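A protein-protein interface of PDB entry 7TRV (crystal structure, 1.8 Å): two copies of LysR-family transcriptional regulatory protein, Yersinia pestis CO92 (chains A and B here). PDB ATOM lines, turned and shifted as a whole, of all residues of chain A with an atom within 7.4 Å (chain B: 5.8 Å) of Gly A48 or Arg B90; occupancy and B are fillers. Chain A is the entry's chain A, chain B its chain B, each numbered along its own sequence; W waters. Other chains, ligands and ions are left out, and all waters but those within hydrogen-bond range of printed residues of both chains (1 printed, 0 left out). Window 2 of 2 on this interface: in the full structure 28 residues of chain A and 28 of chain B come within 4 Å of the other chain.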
ATOM      1  N   SER A   1     -15.335 -31.349  -3.259  1.00  0.00           N
ATOM      2  CA  SER A   1     -15.451 -29.926  -2.964  1.00  0.00           C
ATOM      3  C   SER A   1     -16.540 -29.273  -3.808  1.00  0.00           C
ATOM      4  O   SER A   1     -16.945 -29.807  -4.841  1.00  0.00           O
ATOM      5  CB  SER A   1     -14.117 -29.219  -3.203  1.00  0.00           C
ATOM      6  OG  SER A   1     -13.777 -29.228  -4.579  1.00  0.00           O
ATOM      7  N   LEU A  42     -13.988 -20.312   8.859  1.00  0.00           N
ATOM      8  CA  LEU A  42     -14.861 -21.334   8.290  1.00  0.00           C
ATOM      9  C   LEU A  42     -14.487 -21.653   6.848  1.00  0.00           C
ATOM     10  O   LEU A  42     -14.636 -22.800   6.412  1.00  0.00           O
ATOM     11  CB  LEU A  42     -16.319 -20.887   8.379  1.00  0.00           C
ATOM     12  CG  LEU A  42     -16.915 -20.864   9.786  1.00  0.00           C
ATOM     13  CD1 LEU A  42     -18.386 -20.498   9.735  1.00  0.00           C
ATOM     14  CD2 LEU A  42     -16.717 -22.207  10.467  1.00  0.00           C
ATOM     15  N   LEU A  43     -14.011 -20.657   6.095  1.00  0.00           N
ATOM     16  CA  LEU A  43     -13.532 -20.917   4.742  1.00  0.00           C
ATOM     17  C   LEU A  43     -12.293 -21.802   4.761  1.00  0.00           C
ATOM     18  O   LEU A  43     -12.155 -22.706   3.930  1.00  0.00           O
ATOM     19  CB  LEU A  43     -13.239 -19.599   4.026  1.00  0.00           C
ATOM     20  CG  LEU A  43     -12.543 -19.700   2.666  1.00  0.00           C
ATOM     21  CD1 LEU A  43     -13.402 -20.469   1.678  1.00  0.00           C
ATOM     22  CD2 LEU A  43     -12.209 -18.317   2.129  1.00  0.00           C
ATOM     23  N   GLU A  44     -11.378 -21.549   5.702  1.00  0.00           N
ATOM     24  CA  GLU A  44     -10.219 -22.420   5.862  1.00  0.00           C
ATOM     25  C   GLU A  44     -10.643 -23.850   6.158  1.00  0.00           C
ATOM     26  O   GLU A  44     -10.062 -24.804   5.626  1.00  0.00           O
ATOM     27  CB  GLU A  44      -9.314 -21.896   6.976  1.00  0.00           C
ATOM     28  CG  GLU A  44      -8.265 -20.898   6.529  1.00  0.00           C
ATOM     29  CD  GLU A  44      -7.267 -20.582   7.626  1.00  0.00           C
ATOM     30  OE1 GLU A  44      -7.708 -20.282   8.755  1.00  0.00           O
ATOM     31  OE2 GLU A  44      -6.045 -20.650   7.369  1.00  0.00           O
ATOM     32  N   GLU A  45     -11.666 -24.019   6.998  1.00  0.00           N
ATOM     33  CA  GLU A  45     -12.084 -25.358   7.390  1.00  0.00           C
ATOM     34  C   GLU A  45     -12.776 -26.094   6.248  1.00  0.00           C
ATOM     35  O   GLU A  45     -12.651 -27.320   6.139  1.00  0.00           O
ATOM     36  CB  GLU A  45     -12.994 -25.276   8.612  1.00  0.00           C
ATOM     37  CG  GLU A  45     -13.118 -26.573   9.381  1.00  0.00           C
ATOM     38  CD  GLU A  45     -13.641 -26.363  10.785  1.00  0.00           C
ATOM     39  OE1 GLU A  45     -13.722 -25.194  11.222  1.00  0.00           O
ATOM     40  OE2 GLU A  45     -13.968 -27.367  11.453  1.00  0.00           O
ATOM     41  N   ARG A  46     -13.505 -25.378   5.388  1.00  0.00           N
ATOM     42  CA  ARG A  46     -14.120 -26.031   4.236  1.00  0.00           C
ATOM     43  C   ARG A  46     -13.066 -26.437   3.213  1.00  0.00           C
ATOM     44  O   ARG A  46     -13.071 -27.570   2.717  1.00  0.00           O
ATOM     45  CB  ARG A  46     -15.166 -25.117   3.594  1.00  0.00           C
ATOM     46  CG  ARG A  46     -15.814 -25.728   2.356  1.00  0.00           C
ATOM     47  CD  ARG A  46     -16.880 -24.833   1.746  1.00  0.00           C
ATOM     48  NE  ARG A  46     -16.327 -23.613   1.171  1.00  0.00           N
ATOM     49  CZ  ARG A  46     -15.769 -23.531  -0.029  1.00  0.00           C
ATOM     50  NH1 ARG A  46     -15.633 -24.596  -0.803  1.00  0.00           N
ATOM     51  NH2 ARG A  46     -15.337 -22.352  -0.466  1.00  0.00           N
ATOM     52  N   LEU A  47     -12.151 -25.522   2.884  1.00  0.00           N
ATOM     53  CA  LEU A  47     -11.081 -25.848   1.949  1.00  0.00           C
ATOM     54  C   LEU A  47     -10.126 -26.893   2.510  1.00  0.00           C
ATOM     55  O   LEU A  47      -9.449 -27.575   1.734  1.00  0.00           O
ATOM     56  CB  LEU A  47     -10.303 -24.586   1.574  1.00  0.00           C
ATOM     57  CG  LEU A  47     -11.082 -23.479   0.865  1.00  0.00           C
ATOM     58  CD1 LEU A  47     -10.157 -22.328   0.517  1.00  0.00           C
ATOM     59  CD2 LEU A  47     -11.765 -24.012  -0.382  1.00  0.00           C
ATOM     60  N   GLY A  48     -10.059 -27.036   3.831  1.00  0.00           N
ATOM     61  CA  GLY A  48      -9.177 -28.019   4.430  1.00  0.00           C
ATOM     62  C   GLY A  48      -7.705 -27.692   4.311  1.00  0.00           C
ATOM     63  O   GLY A  48      -6.873 -28.606   4.284  1.00  0.00           O
ATOM     64  N   VAL A  49      -7.358 -26.410   4.231  1.00  0.00           N
ATOM     65  CA  VAL A  49      -5.981 -25.964   4.126  1.00  0.00           C
ATOM     66  C   VAL A  49      -5.756 -24.842   5.135  1.00  0.00           C
ATOM     67  O   VAL A  49      -6.675 -24.405   5.825  1.00  0.00           O
ATOM     68  CB  VAL A  49      -5.622 -25.501   2.698  1.00  0.00           C
ATOM     69  CG1 VAL A  49      -5.723 -26.659   1.717  1.00  0.00           C
ATOM     70  CG2 VAL A  49      -6.523 -24.356   2.272  1.00  0.00           C
ATOM     71  N   ARG A  50      -4.513 -24.386   5.214  1.00  0.00           N
ATOM     72  CA  ARG A  50      -4.119 -23.284   6.085  1.00  0.00           C
ATOM     73  C   ARG A  50      -3.771 -22.102   5.189  1.00  0.00           C
ATOM     74  O   ARG A  50      -2.716 -22.084   4.549  1.00  0.00           O
ATOM     75  CB  ARG A  50      -2.952 -23.692   6.976  1.00  0.00           C
ATOM     76  CG  ARG A  50      -2.402 -22.587   7.858  1.00  0.00           C
ATOM     77  CD  ARG A  50      -1.299 -23.131   8.751  1.00  0.00           C
ATOM     78  NE  ARG A  50      -0.257 -23.802   7.981  1.00  0.00           N
ATOM     79  CZ  ARG A  50       0.937 -23.286   7.723  1.00  0.00           C
ATOM     80  NH1 ARG A  50       1.293 -22.100   8.188  1.00  0.00           N
ATOM     81  NH2 ARG A  50       1.799 -23.982   6.985  1.00  0.00           N
ATOM     82  N   LEU A  51      -4.670 -21.122   5.134  1.00  0.00           N
ATOM     83  CA  LEU A  51      -4.455 -19.947   4.305  1.00  0.00           C
ATOM     84  C   LEU A  51      -3.703 -18.844   5.031  1.00  0.00           C
ATOM     85  O   LEU A  51      -3.009 -18.049   4.388  1.00  0.00           O
ATOM     86  CB  LEU A  51      -5.795 -19.393   3.816  1.00  0.00           C
ATOM     87  CG  LEU A  51      -6.724 -20.318   3.024  1.00  0.00           C
ATOM     88  CD1 LEU A  51      -8.082 -19.655   2.820  1.00  0.00           C
ATOM     89  CD2 LEU A  51      -6.103 -20.692   1.688  1.00  0.00           C
ATOM     90  N   SER B  85      -7.318 -24.573  -7.400  1.00  0.00           N
ATOM     91  CA  SER B  85      -6.018 -24.322  -6.792  1.00  0.00           C
ATOM     92  C   SER B  85      -5.923 -24.909  -5.389  1.00  0.00           C
ATOM     93  O   SER B  85      -4.811 -25.148  -4.905  1.00  0.00           O
ATOM     94  CB  SER B  85      -5.721 -22.818  -6.763  1.00  0.00           C
ATOM     95  OG  SER B  85      -6.641 -22.116  -5.940  1.00  0.00           O
ATOM     96  N   ILE B  86      -7.054 -25.147  -4.732  1.00  0.00           N
ATOM     97  CA  ILE B  86      -7.068 -25.856  -3.456  1.00  0.00           C
ATOM     98  C   ILE B  86      -7.086 -27.364  -3.664  1.00  0.00           C
ATOM     99  O   ILE B  86      -6.336 -28.100  -3.017  1.00  0.00           O
ATOM    100  CB  ILE B  86      -8.276 -25.400  -2.610  1.00  0.00           C
ATOM    101  CG1 ILE B  86      -8.209 -23.900  -2.330  1.00  0.00           C
ATOM    102  CG2 ILE B  86      -8.349 -26.197  -1.316  1.00  0.00           C
ATOM    103  CD1 ILE B  86      -7.027 -23.481  -1.489  1.00  0.00           C
ATOM    104  N   ASP B  87      -7.945 -27.841  -4.571  1.00  0.00           N
ATOM    105  CA  ASP B  87      -8.026 -29.273  -4.834  1.00  0.00           C
ATOM    106  C   ASP B  87      -6.705 -29.820  -5.351  1.00  0.00           C
ATOM    107  O   ASP B  87      -6.348 -30.965  -5.053  1.00  0.00           O
ATOM    108  CB  ASP B  87      -9.147 -29.562  -5.828  1.00  0.00           C
ATOM    109  CG  ASP B  87     -10.513 -29.179  -5.294  1.00  0.00           C
ATOM    110  OD1 ASP B  87     -10.600 -28.743  -4.128  1.00  0.00           O
ATOM    111  OD2 ASP B  87     -11.500 -29.313  -6.048  1.00  0.00           O
ATOM    112  N   LEU B  88      -5.966 -29.020  -6.122  1.00  0.00           N
ATOM    113  CA  LEU B  88      -4.645 -29.443  -6.579  1.00  0.00           C
ATOM    114  C   LEU B  88      -3.672 -29.557  -5.411  1.00  0.00           C
ATOM    115  O   LEU B  88      -2.856 -30.485  -5.365  1.00  0.00           O
ATOM    116  CB  LEU B  88      -4.117 -28.467  -7.630  1.00  0.00           C
ATOM    117  CG  LEU B  88      -2.685 -28.691  -8.115  1.00  0.00           C
ATOM    118  CD1 LEU B  88      -2.533 -30.067  -8.750  1.00  0.00           C
ATOM    119  CD2 LEU B  88      -2.267 -27.598  -9.088  1.00  0.00           C
ATOM    120  N   THR B  89      -3.747 -28.625  -4.458  1.00  0.00           N
ATOM    121  CA  THR B  89      -2.886 -28.695  -3.281  1.00  0.00           C
ATOM    122  C   THR B  89      -3.251 -29.879  -2.391  1.00  0.00           C
ATOM    123  O   THR B  89      -2.386 -30.421  -1.692  1.00  0.00           O
ATOM    124  CB  THR B  89      -2.970 -27.386  -2.493  1.00  0.00           C
ATOM    125  OG1 THR B  89      -2.685 -26.285  -3.366  1.00  0.00           O
ATOM    126  CG2 THR B  89      -1.973 -27.376  -1.346  1.00  0.00           C
ATOM    127  N   ARG B  90      -4.509 -30.301  -2.412  1.00  0.00           N
ATOM    128  CA  ARG B  90      -4.938 -31.425  -1.591  1.00  0.00           C
ATOM    129  C   ARG B  90      -5.342 -32.615  -2.453  1.00  0.00           C
ATOM    130  O   ARG B  90      -4.812 -33.715  -2.291  1.00  0.00           O
ATOM    131  CB  ARG B  90      -6.098 -31.011  -0.685  1.00  0.00           C
ATOM    132  CG  ARG B  90      -7.383 -30.685  -1.424  1.00  0.00           C
ATOM    133  CD  ARG B  90      -8.479 -30.314  -0.443  1.00  0.00           C
ATOM    134  NE  ARG B  90      -8.507 -31.228   0.692  1.00  0.00           N
ATOM    135  CZ  ARG B  90      -9.420 -31.207   1.653  1.00  0.00           C
ATOM    136  NH1 ARG B  90     -10.415 -30.336   1.641  1.00  0.00           N
ATOM    137  NH2 ARG B  90      -9.335 -32.086   2.649  1.00  0.00           N
HETATM  138  O   HOH W   1     -11.266 -28.274  -0.869  1.00  0.00           O
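The backbone carbonyl oxygen (O) of Leu A47 lies within hydrogen-bond range of the guanidinium group (NH1) of Arg B90. The side-chain hydroxyl (OG) of Ser A1 is in hydrogen-bond range of the side-chain carboxylate (OD2) of Asp B87 (2.7 Å).
The backbone NH (N) of Val A49 lies within hydrogen-bond range of the backbone carbonyl oxygen (O) of Glu A44 (3.4 Å).
Among the printed residues, merely in contact across the chains: Arg A46 with Arg B90 (3.98 Å), Leu A47 with Ile B86 (3.5 Å), Gly A48 with Arg B90 (3.8 Å) and Val A49 with Ile B86 (3.9 Å).
Of the printed residues of chain B, Ser A1 touches Asp B87. Glu A45 touches none of the printed residues of chain B. Gly A48 touches just one residue of chain B: Arg B90. Of the printed residues of chain B, Val A49 touches Ile B86. Leu A51 touches none of the printed residues of chain B. Of the printed residues of chain A, Asp B87 touches Ser A1. Printed residues of chain A within 4 Å of Arg B90: Arg A46 (3.98 Å), Leu A47 (2.9 Å) and Gly A48 (3.8 Å).
Of the 6 printed residues of chain B, 3 touch a printed residue of chain A. Printed residues of chain B that touch a printed residue of chain A: Ile B86, Asp B87 and Arg B90. Hydrophobic or aromatic side chains of chain B that line the printed part of chain A: Ile B86.
No position is printed for both chains.
Water W1 lies within hydrogen-bond range of O of Leu A47 (3.3 Å), NH1 of Arg B90 (3.4 Å) and OD1 of Asp B87 (3.4 Å).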
